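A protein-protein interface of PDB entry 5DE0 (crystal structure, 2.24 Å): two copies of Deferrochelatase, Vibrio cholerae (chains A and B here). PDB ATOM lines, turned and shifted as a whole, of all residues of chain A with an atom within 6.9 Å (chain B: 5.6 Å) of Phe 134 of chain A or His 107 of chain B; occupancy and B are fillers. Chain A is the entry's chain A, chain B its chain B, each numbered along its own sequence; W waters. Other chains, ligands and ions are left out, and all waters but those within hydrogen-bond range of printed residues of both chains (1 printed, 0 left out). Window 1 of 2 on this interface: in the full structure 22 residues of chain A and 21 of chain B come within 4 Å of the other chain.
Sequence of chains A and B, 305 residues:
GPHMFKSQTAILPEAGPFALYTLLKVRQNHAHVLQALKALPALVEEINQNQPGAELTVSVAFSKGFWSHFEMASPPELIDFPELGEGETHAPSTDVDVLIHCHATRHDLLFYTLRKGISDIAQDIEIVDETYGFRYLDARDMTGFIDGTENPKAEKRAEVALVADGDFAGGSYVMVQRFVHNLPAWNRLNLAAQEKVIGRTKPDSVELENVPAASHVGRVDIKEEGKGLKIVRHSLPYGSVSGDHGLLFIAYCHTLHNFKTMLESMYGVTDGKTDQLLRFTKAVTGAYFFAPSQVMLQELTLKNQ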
ATOM      1  N   GLY A  16      17.843  -5.348   4.099  1.00  0.00           N
ATOM      2  CA  GLY A  16      18.757  -5.326   2.972  1.00  0.00           C
ATOM      3  C   GLY A  16      19.224  -3.917   2.651  1.00  0.00           C
ATOM      4  O   GLY A  16      18.731  -2.950   3.235  1.00  0.00           O
ATOM      5  N   PRO A  17      20.183  -3.791   1.719  1.00  0.00           N
ATOM      6  CA  PRO A  17      20.723  -2.495   1.290  1.00  0.00           C
ATOM      7  C   PRO A  17      19.661  -1.575   0.687  1.00  0.00           C
ATOM      8  O   PRO A  17      19.854  -0.360   0.644  1.00  0.00           O
ATOM      9  CB  PRO A  17      21.766  -2.881   0.234  1.00  0.00           C
ATOM     10  CG  PRO A  17      22.142  -4.282   0.569  1.00  0.00           C
ATOM     11  CD  PRO A  17      20.890  -4.918   1.089  1.00  0.00           C
ATOM     12  N   PHE A  18      18.558  -2.153   0.226  1.00  0.00           N
ATOM     13  CA  PHE A  18      17.468  -1.377  -0.354  1.00  0.00           C
ATOM     14  C   PHE A  18      16.127  -1.838   0.201  1.00  0.00           C
ATOM     15  O   PHE A  18      15.928  -3.027   0.445  1.00  0.00           O
ATOM     16  CB  PHE A  18      17.477  -1.492  -1.878  1.00  0.00           C
ATOM     17  CG  PHE A  18      18.770  -1.064  -2.510  1.00  0.00           C
ATOM     18  CD1 PHE A  18      19.042   0.277  -2.726  1.00  0.00           C
ATOM     19  CD2 PHE A  18      19.712  -2.005  -2.893  1.00  0.00           C
ATOM     20  CE1 PHE A  18      20.230   0.672  -3.308  1.00  0.00           C
ATOM     21  CE2 PHE A  18      20.903  -1.616  -3.477  1.00  0.00           C
ATOM     22  CZ  PHE A  18      21.162  -0.275  -3.685  1.00  0.00           C
ATOM     23  N   ALA A  19      15.209  -0.896   0.398  1.00  0.00           N
ATOM     24  CA  ALA A  19      13.908  -1.219   0.974  1.00  0.00           C
ATOM     25  C   ALA A  19      12.778  -0.394   0.363  1.00  0.00           C
ATOM     26  O   ALA A  19      12.985   0.740  -0.077  1.00  0.00           O
ATOM     27  CB  ALA A  19      13.943  -1.023   2.481  1.00  0.00           C
ATOM     28  N   TYR A  21       8.766   0.970   1.138  1.00  0.00           N
ATOM     29  CA  TYR A  21       7.730   1.173   2.141  1.00  0.00           C
ATOM     30  C   TYR A  21       6.519   1.856   1.516  1.00  0.00           C
ATOM     31  O   TYR A  21       6.588   3.025   1.136  1.00  0.00           O
ATOM     32  CB  TYR A  21       8.253   2.013   3.306  1.00  0.00           C
ATOM     33  CG  TYR A  21       9.630   1.633   3.808  1.00  0.00           C
ATOM     34  CD1 TYR A  21       9.792   0.647   4.772  1.00  0.00           C
ATOM     35  CD2 TYR A  21      10.766   2.282   3.337  1.00  0.00           C
ATOM     36  CE1 TYR A  21      11.049   0.305   5.242  1.00  0.00           C
ATOM     37  CE2 TYR A  21      12.024   1.951   3.805  1.00  0.00           C
ATOM     38  CZ  TYR A  21      12.161   0.961   4.758  1.00  0.00           C
ATOM     39  OH  TYR A  21      13.409   0.625   5.226  1.00  0.00           O
ATOM     40  N   HIS A 107      17.707  -2.777  -5.867  1.00  0.00           N
ATOM     41  CA  HIS A 107      16.662  -1.760  -5.872  1.00  0.00           C
ATOM     42  C   HIS A 107      15.601  -1.998  -6.944  1.00  0.00           C
ATOM     43  O   HIS A 107      14.415  -1.756  -6.714  1.00  0.00           O
ATOM     44  CB  HIS A 107      17.289  -0.378  -6.067  1.00  0.00           C
ATOM     45  CG  HIS A 107      16.294   0.707  -6.331  1.00  0.00           C
ATOM     46  ND1 HIS A 107      15.644   1.384  -5.321  1.00  0.00           N
ATOM     47  CD2 HIS A 107      15.833   1.233  -7.490  1.00  0.00           C
ATOM     48  CE1 HIS A 107      14.829   2.280  -5.846  1.00  0.00           C
ATOM     49  NE2 HIS A 107      14.924   2.208  -7.162  1.00  0.00           N
ATOM     50  N   TYR A 132      11.317   4.727  -1.106  1.00  0.00           N
ATOM     51  CA  TYR A 132      12.406   3.802  -1.394  1.00  0.00           C
ATOM     52  C   TYR A 132      13.613   4.104  -0.516  1.00  0.00           C
ATOM     53  O   TYR A 132      14.319   5.091  -0.731  1.00  0.00           O
ATOM     54  CB  TYR A 132      12.798   3.869  -2.872  1.00  0.00           C
ATOM     55  CG  TYR A 132      11.772   3.255  -3.794  1.00  0.00           C
ATOM     56  CD1 TYR A 132      10.700   4.001  -4.266  1.00  0.00           C
ATOM     57  CD2 TYR A 132      11.872   1.927  -4.189  1.00  0.00           C
ATOM     58  CE1 TYR A 132       9.758   3.443  -5.108  1.00  0.00           C
ATOM     59  CE2 TYR A 132      10.935   1.360  -5.032  1.00  0.00           C
ATOM     60  CZ  TYR A 132       9.880   2.121  -5.487  1.00  0.00           C
ATOM     61  OH  TYR A 132       8.943   1.562  -6.325  1.00  0.00           O
ATOM     62  N   GLY A 133      13.842   3.249   0.473  1.00  0.00           N
ATOM     63  CA  GLY A 133      14.964   3.418   1.375  1.00  0.00           C
ATOM     64  C   GLY A 133      16.241   2.798   0.843  1.00  0.00           C
ATOM     65  O   GLY A 133      16.206   1.891   0.013  1.00  0.00           O
ATOM     66  N   PHE A 134      17.376   3.296   1.320  1.00  0.00           N
ATOM     67  CA  PHE A 134      18.674   2.735   0.963  1.00  0.00           C
ATOM     68  C   PHE A 134      19.664   2.928   2.103  1.00  0.00           C
ATOM     69  O   PHE A 134      19.696   3.982   2.736  1.00  0.00           O
ATOM     70  CB  PHE A 134      19.211   3.367  -0.324  1.00  0.00           C
ATOM     71  CG  PHE A 134      19.273   4.870  -0.288  1.00  0.00           C
ATOM     72  CD1 PHE A 134      20.417   5.520   0.148  1.00  0.00           C
ATOM     73  CD2 PHE A 134      18.193   5.632  -0.703  1.00  0.00           C
ATOM     74  CE1 PHE A 134      20.477   6.900   0.180  1.00  0.00           C
ATOM     75  CE2 PHE A 134      18.248   7.013  -0.674  1.00  0.00           C
ATOM     76  CZ  PHE A 134      19.392   7.648  -0.234  1.00  0.00           C
ATOM     77  N   ARG A 135      20.463   1.900   2.370  1.00  0.00           N
ATOM     78  CA  ARG A 135      21.499   1.995   3.385  1.00  0.00           C
ATOM     79  C   ARG A 135      22.535   3.017   2.937  1.00  0.00           C
ATOM     80  O   ARG A 135      23.024   2.965   1.808  1.00  0.00           O
ATOM     81  CB  ARG A 135      22.143   0.632   3.643  1.00  0.00           C
ATOM     82  CG  ARG A 135      23.065   0.603   4.847  1.00  0.00           C
ATOM     83  CD  ARG A 135      23.349  -0.821   5.285  1.00  0.00           C
ATOM     84  NE  ARG A 135      22.196  -1.441   5.931  1.00  0.00           N
ATOM     85  CZ  ARG A 135      21.814  -2.699   5.733  1.00  0.00           C
ATOM     86  NH1 ARG A 135      22.490  -3.478   4.899  1.00  0.00           N
ATOM     87  NH2 ARG A 135      20.753  -3.178   6.368  1.00  0.00           N
ATOM     88  N   TYR A 136      22.855   3.951   3.826  1.00  0.00           N
ATOM     89  CA  TYR A 136      23.660   5.114   3.474  1.00  0.00           C
ATOM     90  C   TYR A 136      25.029   5.073   4.145  1.00  0.00           C
ATOM     91  O   TYR A 136      25.128   5.154   5.370  1.00  0.00           O
ATOM     92  CB  TYR A 136      22.910   6.392   3.856  1.00  0.00           C
ATOM     93  CG  TYR A 136      23.596   7.675   3.459  1.00  0.00           C
ATOM     94  CD1 TYR A 136      23.711   8.044   2.124  1.00  0.00           C
ATOM     95  CD2 TYR A 136      24.108   8.532   4.422  1.00  0.00           C
ATOM     96  CE1 TYR A 136      24.331   9.224   1.761  1.00  0.00           C
ATOM     97  CE2 TYR A 136      24.728   9.715   4.069  1.00  0.00           C
ATOM     98  CZ  TYR A 136      24.838  10.057   2.738  1.00  0.00           C
ATOM     99  OH  TYR A 136      25.456  11.235   2.388  1.00  0.00           O
ATOM    100  N   LEU A 137      26.074   4.959   3.327  1.00  0.00           N
ATOM    101  CA  LEU A 137      27.444   4.787   3.808  1.00  0.00           C
ATOM    102  C   LEU A 137      27.518   3.590   4.751  1.00  0.00           C
ATOM    103  O   LEU A 137      26.918   2.554   4.482  1.00  0.00           O
ATOM    104  CB  LEU A 137      27.945   6.059   4.497  1.00  0.00           C
ATOM    105  CG  LEU A 137      27.798   7.338   3.671  1.00  0.00           C
ATOM    106  CD1 LEU A 137      28.341   8.539   4.430  1.00  0.00           C
ATOM    107  CD2 LEU A 137      28.485   7.194   2.319  1.00  0.00           C
ATOM    108  N   ARG A 140      24.611   4.661   8.135  1.00  0.00           N
ATOM    109  CA  ARG A 140      24.410   5.952   8.777  1.00  0.00           C
ATOM    110  C   ARG A 140      23.118   6.630   8.338  1.00  0.00           C
ATOM    111  O   ARG A 140      22.684   6.490   7.194  1.00  0.00           O
ATOM    112  CB  ARG A 140      25.595   6.877   8.491  1.00  0.00           C
ATOM    113  CG  ARG A 140      26.950   6.221   8.662  1.00  0.00           C
ATOM    114  CD  ARG A 140      28.057   7.257   8.684  1.00  0.00           C
ATOM    115  NE  ARG A 140      28.140   7.936   9.971  1.00  0.00           N
ATOM    116  CZ  ARG A 140      29.005   7.622  10.929  1.00  0.00           C
ATOM    117  NH1 ARG A 140      29.873   6.635  10.750  1.00  0.00           N
ATOM    118  NH2 ARG A 140      29.003   8.299  12.067  1.00  0.00           N
ATOM    119  N   MET A 142      21.177  10.254   7.556  1.00  0.00           N
ATOM    120  CA  MET A 142      21.664  11.427   6.833  1.00  0.00           C
ATOM    121  C   MET A 142      22.074  12.571   7.759  1.00  0.00           C
ATOM    122  O   MET A 142      22.582  13.593   7.301  1.00  0.00           O
ATOM    123  CB  MET A 142      20.605  11.905   5.838  1.00  0.00           C
ATOM    124  CG  MET A 142      20.433  10.969   4.655  1.00  0.00           C
ATOM    125  SD  MET A 142      19.056  11.399   3.583  1.00  0.00           S
ATOM    126  CE  MET A 142      19.225  10.152   2.310  1.00  0.00           C
ATOM    127  N   LEU A 236      15.345   3.037   7.319  1.00  0.00           N
ATOM    128  CA  LEU A 236      16.363   3.263   6.302  1.00  0.00           C
ATOM    129  C   LEU A 236      16.229   4.667   5.715  1.00  0.00           C
ATOM    130  O   LEU A 236      15.114   5.151   5.517  1.00  0.00           O
ATOM    131  CB  LEU A 236      16.250   2.210   5.197  1.00  0.00           C
ATOM    132  CG  LEU A 236      17.543   1.605   4.649  1.00  0.00           C
ATOM    133  CD1 LEU A 236      18.380   1.015   5.773  1.00  0.00           C
ATOM    134  CD2 LEU A 236      17.225   0.545   3.605  1.00  0.00           C
ATOM    135  N   PRO A 237      17.366   5.331   5.452  1.00  0.00           N
ATOM    136  CA  PRO A 237      17.386   6.665   4.837  1.00  0.00           C
ATOM    137  C   PRO A 237      16.704   6.694   3.466  1.00  0.00           C
ATOM    138  O   PRO A 237      16.624   5.665   2.795  1.00  0.00           O
ATOM    139  CB  PRO A 237      18.882   6.968   4.709  1.00  0.00           C
ATOM    140  CG  PRO A 237      19.526   6.144   5.764  1.00  0.00           C
ATOM    141  CD  PRO A 237      18.716   4.881   5.831  1.00  0.00           C
ATOM    142  N   TYR A 238      16.229   7.866   3.057  1.00  0.00           N
ATOM    143  CA  TYR A 238      15.500   8.000   1.801  1.00  0.00           C
ATOM    144  C   TYR A 238      15.585   9.419   1.252  1.00  0.00           C
ATOM    145  O   TYR A 238      16.043  10.333   1.935  1.00  0.00           O
ATOM    146  CB  TYR A 238      14.028   7.629   1.995  1.00  0.00           C
ATOM    147  CG  TYR A 238      13.202   8.775   2.543  1.00  0.00           C
ATOM    148  CD1 TYR A 238      13.249   9.110   3.890  1.00  0.00           C
ATOM    149  CD2 TYR A 238      12.383   9.531   1.710  1.00  0.00           C
ATOM    150  CE1 TYR A 238      12.503  10.161   4.393  1.00  0.00           C
ATOM    151  CE2 TYR A 238      11.636  10.583   2.203  1.00  0.00           C
ATOM    152  CZ  TYR A 238      11.698  10.894   3.544  1.00  0.00           C
ATOM    153  OH  TYR A 238      10.952  11.941   4.035  1.00  0.00           O
ATOM    154  N   GLY A 239      15.128   9.595   0.016  1.00  0.00           N
ATOM    155  CA  GLY A 239      14.890  10.920  -0.524  1.00  0.00           C
ATOM    156  C   GLY A 239      15.966  11.499  -1.418  1.00  0.00           C
ATOM    157  O   GLY A 239      16.959  10.842  -1.736  1.00  0.00           O
ATOM    158  N   SER A 240      15.754  12.747  -1.823  1.00  0.00           N
ATOM    159  CA  SER A 240      16.681  13.453  -2.696  1.00  0.00           C
ATOM    160  C   SER A 240      17.204  14.713  -2.022  1.00  0.00           C
ATOM    161  O   SER A 240      16.661  15.163  -1.013  1.00  0.00           O
ATOM    162  CB  SER A 240      16.003  13.809  -4.021  1.00  0.00           C
ATOM    163  OG  SER A 240      14.897  14.668  -3.808  1.00  0.00           O
ATOM    164  N   GLY A 246      15.501  12.147   4.513  1.00  0.00           N
ATOM    165  CA  GLY A 246      15.607  11.857   5.929  1.00  0.00           C
ATOM    166  C   GLY A 246      15.583  10.369   6.204  1.00  0.00           C
ATOM    167  O   GLY A 246      16.336   9.606   5.602  1.00  0.00           O
ATOM    168  N   PHE B  18      23.812   2.158 -11.025  1.00  0.00           N
ATOM    169  CA  PHE B  18      23.090   3.324 -10.529  1.00  0.00           C
ATOM    170  C   PHE B  18      23.697   4.599 -11.092  1.00  0.00           C
ATOM    171  O   PHE B  18      24.904   4.668 -11.314  1.00  0.00           O
ATOM    172  CB  PHE B  18      23.114   3.371  -9.001  1.00  0.00           C
ATOM    173  CG  PHE B  18      22.656   2.102  -8.351  1.00  0.00           C
ATOM    174  CD1 PHE B  18      21.316   1.902  -8.068  1.00  0.00           C
ATOM    175  CD2 PHE B  18      23.565   1.106  -8.025  1.00  0.00           C
ATOM    176  CE1 PHE B  18      20.888   0.728  -7.467  1.00  0.00           C
ATOM    177  CE2 PHE B  18      23.144  -0.068  -7.426  1.00  0.00           C
ATOM    178  CZ  PHE B  18      21.803  -0.257  -7.145  1.00  0.00           C
ATOM    179  N   THR B 105      28.645   1.798  -8.799  1.00  0.00           N
ATOM    180  CA  THR B 105      28.153   0.457  -8.501  1.00  0.00           C
ATOM    181  C   THR B 105      27.274   0.455  -7.254  1.00  0.00           C
ATOM    182  O   THR B 105      26.741  -0.585  -6.864  1.00  0.00           O
ATOM    183  CB  THR B 105      29.310  -0.547  -8.305  1.00  0.00           C
ATOM    184  OG1 THR B 105      30.127  -0.135  -7.203  1.00  0.00           O
ATOM    185  CG2 THR B 105      30.165  -0.627  -9.561  1.00  0.00           C
ATOM    186  N   ARG B 106      27.125   1.621  -6.634  1.00  0.00           N
ATOM    187  CA  ARG B 106      26.248   1.760  -5.474  1.00  0.00           C
ATOM    188  C   ARG B 106      25.503   3.091  -5.510  1.00  0.00           C
ATOM    189  O   ARG B 106      25.999   4.084  -6.046  1.00  0.00           O
ATOM    190  CB  ARG B 106      27.043   1.615  -4.171  1.00  0.00           C
ATOM    191  CG  ARG B 106      28.411   2.271  -4.192  1.00  0.00           C
ATOM    192  CD  ARG B 106      29.255   1.850  -2.993  1.00  0.00           C
ATOM    193  NE  ARG B 106      28.779   2.430  -1.739  1.00  0.00           N
ATOM    194  CZ  ARG B 106      29.491   2.462  -0.617  1.00  0.00           C
ATOM    195  NH1 ARG B 106      30.715   1.951  -0.591  1.00  0.00           N
ATOM    196  NH2 ARG B 106      28.987   3.010   0.480  1.00  0.00           N
ATOM    197  N   HIS B 107      24.307   3.098  -4.933  1.00  0.00           N
ATOM    198  CA  HIS B 107      23.407   4.242  -5.019  1.00  0.00           C
ATOM    199  C   HIS B 107      23.731   5.340  -4.008  1.00  0.00           C
ATOM    200  O   HIS B 107      23.651   6.525  -4.329  1.00  0.00           O
ATOM    201  CB  HIS B 107      21.960   3.772  -4.834  1.00  0.00           C
ATOM    202  CG  HIS B 107      20.969   4.886  -4.693  1.00  0.00           C
ATOM    203  ND1 HIS B 107      20.337   5.460  -5.775  1.00  0.00           N
ATOM    204  CD2 HIS B 107      20.499   5.528  -3.598  1.00  0.00           C
ATOM    205  CE1 HIS B 107      19.521   6.409  -5.352  1.00  0.00           C
ATOM    206  NE2 HIS B 107      19.601   6.471  -4.035  1.00  0.00           N
ATOM    207  N   ASP B 108      24.095   4.942  -2.792  1.00  0.00           N
ATOM    208  CA  ASP B 108      24.254   5.887  -1.687  1.00  0.00           C
ATOM    209  C   ASP B 108      25.318   6.957  -1.946  1.00  0.00           C
ATOM    210  O   ASP B 108      25.126   8.122  -1.596  1.00  0.00           O
ATOM    211  CB  ASP B 108      24.578   5.134  -0.390  1.00  0.00           C
ATOM    212  CG  ASP B 108      25.882   4.362  -0.466  1.00  0.00           C
ATOM    213  OD1 ASP B 108      26.222   3.856  -1.559  1.00  0.00           O
ATOM    214  OD2 ASP B 108      26.568   4.265   0.573  1.00  0.00           O
ATOM    215  N   LEU B 109      26.427   6.569  -2.570  1.00  0.00           N
ATOM    216  CA  LEU B 109      27.518   7.506  -2.827  1.00  0.00           C
ATOM    217  C   LEU B 109      27.129   8.591  -3.833  1.00  0.00           C
ATOM    218  O   LEU B 109      27.758   9.649  -3.887  1.00  0.00           O
ATOM    219  CB  LEU B 109      28.758   6.760  -3.320  1.00  0.00           C
ATOM    220  CG  LEU B 109      29.457   5.873  -2.288  1.00  0.00           C
ATOM    221  CD1 LEU B 109      30.657   5.189  -2.911  1.00  0.00           C
ATOM    222  CD2 LEU B 109      29.874   6.690  -1.071  1.00  0.00           C
ATOM    223  N   LEU B 110      26.095   8.323  -4.627  1.00  0.00           N
ATOM    224  CA  LEU B 110      25.576   9.312  -5.566  1.00  0.00           C
ATOM    225  C   LEU B 110      24.907  10.452  -4.810  1.00  0.00           C
ATOM    226  O   LEU B 110      25.150  11.626  -5.090  1.00  0.00           O
ATOM    227  CB  LEU B 110      24.582   8.673  -6.539  1.00  0.00           C
ATOM    228  CG  LEU B 110      25.091   7.511  -7.393  1.00  0.00           C
ATOM    229  CD1 LEU B 110      23.954   6.943  -8.226  1.00  0.00           C
ATOM    230  CD2 LEU B 110      26.245   7.950  -8.281  1.00  0.00           C
ATOM    231  N   PHE B 111      24.059  10.094  -3.852  1.00  0.00           N
ATOM    232  CA  PHE B 111      23.417  11.075  -2.990  1.00  0.00           C
ATOM    233  C   PHE B 111      24.466  11.857  -2.207  1.00  0.00           C
ATOM    234  O   PHE B 111      24.368  13.077  -2.073  1.00  0.00           O
ATOM    235  CB  PHE B 111      22.433  10.393  -2.032  1.00  0.00           C
ATOM    236  CG  PHE B 111      21.710  11.348  -1.119  1.00  0.00           C
ATOM    237  CD1 PHE B 111      22.270  11.738   0.089  1.00  0.00           C
ATOM    238  CD2 PHE B 111      20.467  11.851  -1.468  1.00  0.00           C
ATOM    239  CE1 PHE B 111      21.610  12.615   0.923  1.00  0.00           C
ATOM    240  CE2 PHE B 111      19.799  12.726  -0.635  1.00  0.00           C
ATOM    241  CZ  PHE B 111      20.371  13.109   0.563  1.00  0.00           C
ATOM    242  N   TYR B 132      17.545  10.024 -10.002  1.00  0.00           N
ATOM    243  CA  TYR B 132      18.375   8.875  -9.667  1.00  0.00           C
ATOM    244  C   TYR B 132      17.981   7.673 -10.515  1.00  0.00           C
ATOM    245  O   TYR B 132      16.907   7.097 -10.330  1.00  0.00           O
ATOM    246  CB  TYR B 132      18.256   8.539  -8.180  1.00  0.00           C
ATOM    247  CG  TYR B 132      18.887   9.571  -7.269  1.00  0.00           C
ATOM    248  CD1 TYR B 132      18.153  10.655  -6.802  1.00  0.00           C
ATOM    249  CD2 TYR B 132      20.215   9.462  -6.880  1.00  0.00           C
ATOM    250  CE1 TYR B 132      18.723  11.600  -5.972  1.00  0.00           C
ATOM    251  CE2 TYR B 132      20.794  10.404  -6.049  1.00  0.00           C
ATOM    252  CZ  TYR B 132      20.043  11.470  -5.599  1.00  0.00           C
ATOM    253  OH  TYR B 132      20.615  12.410  -4.773  1.00  0.00           O
ATOM    254  N   GLY B 133      18.855   7.303 -11.445  1.00  0.00           N
ATOM    255  CA  GLY B 133      18.595   6.188 -12.334  1.00  0.00           C
ATOM    256  C   GLY B 133      19.118   4.880 -11.775  1.00  0.00           C
ATOM    257  O   GLY B 133      20.029   4.866 -10.945  1.00  0.00           O
HETATM  258  O   HOH W   1      17.855   9.032  -3.638  1.00  0.00           O
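Of chain B, only His 107 comes within 4 Å of Phe 134 of chain A.
Of the printed residues of chain B, Tyr 136 of chain A touches Asp 108 and Phe 111.
Printed residues of chain B within 4 Å of Met 142 of chain A: Phe 111 (3.6 Å).
Of the printed residues of chain A, Phe 18 of chain B touches Phe 18.
Of chain A, only Phe 18 and Phe 134 come within 4 Å of His 107 of chain B.
The nearest residue of chain B that does not touch Phe 134 of chain A is Asp 108 of chain B (4.2 Å).
The nearest residue of chain A that does not touch His 107 of chain B is Gly 239 of chain A (5.6 Å).
The nearest printed residue of chain A that does not touch Phe 111 of chain B is Phe 134 of chain A (4.5 Å).
Water W1 lies within hydrogen-bond range of the backbone carbonyl oxygen of Gly 239 of chain A (2.8 Å) and a ring nitrogen (NE2) of His 107 of chain B (3.1 Å).
Phe 18 of chain B touches Phe 18 of chain A.
His 107 of chain B touches Phe 18 of chain A.
His 107 of chain B touches Phe 134 of chain A (CD2 to CG, 3.6 Å).
Arg 135 of chain A touches Asp 108 of chain B.
Asp 108 of chain B touches Tyr 136 of chain A (O to CE1, 3.6 Å).
Phe 111 of chain B touches Tyr 136 of chain A (CD1 to CE1, 3.7 Å).
Leu 137 of chain A touches Leu 109 of chain B (CD2 to CD2, 3.7 Å).
Met 142 of chain A touches Phe 111 of chain B.
Gly 239 of chain A touches Phe 111 of chain B (O to CE2, 3.6 Å).
CE2 of Phe 111 of chain B touches C of Ser 240 of chain A (3.6 Å).
Printed residues of chain A that touch a printed residue of chain B: Phe 18, Phe 134, Arg 135, Tyr 136, Leu 137, Met 142, Gly 239 and Ser 240.
Printed residues of chain B that touch a printed residue of chain A: Phe 18, His 107, Asp 108, Leu 109 and Phe 111.
Hydrophobic or aromatic side chains of chain B within 4 Å of the printed part of chain A: Phe 18, His 107, Leu 109 and Phe 111.
Among the printed residues, no Asp or Glu carboxylate lies within 4 Å of a Lys or Arg side-chain nitrogen of the other chain.
The backbone NH (N) of Leu 137 of chain A sits at hydrogen-bond distance from the side-chain carboxylate (OD2) of Asp 108 of chain B, 2.9 Å away.
NH2 of Arg 106 of chain B is in salt-bridge range of OD2 of Asp 108 of chain B (2.7 Å).
SD of Met 142 of chain A sits at hydrogen-bond distance from N of Gly 246 of chain A (3.7 Å).
The backbone carbonyl oxygen (O) of Pro 237 of chain A sits at hydrogen-bond distance from the backbone NH (N) of Phe 134 of chain A.
The backbone carbonyl oxygen (O) of Pro 17 of chain A sits at hydrogen-bond distance from the backbone NH (N) of Arg 135 of chain A (2.9 Å).
Phe 18 of chain B touches its own counterpart, Phe 18 of chain A.
Phe 18 of chain A touches His 107 of chain B, but with the chains exchanged His 107 of chain A does not touch Phe 18 of chain B (4.02 Å).
4 positions are printed for both chains.
Of the 11 pairs that touch across the chains among the printed residues, 1 has its exchanged pair printed and touching as well.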
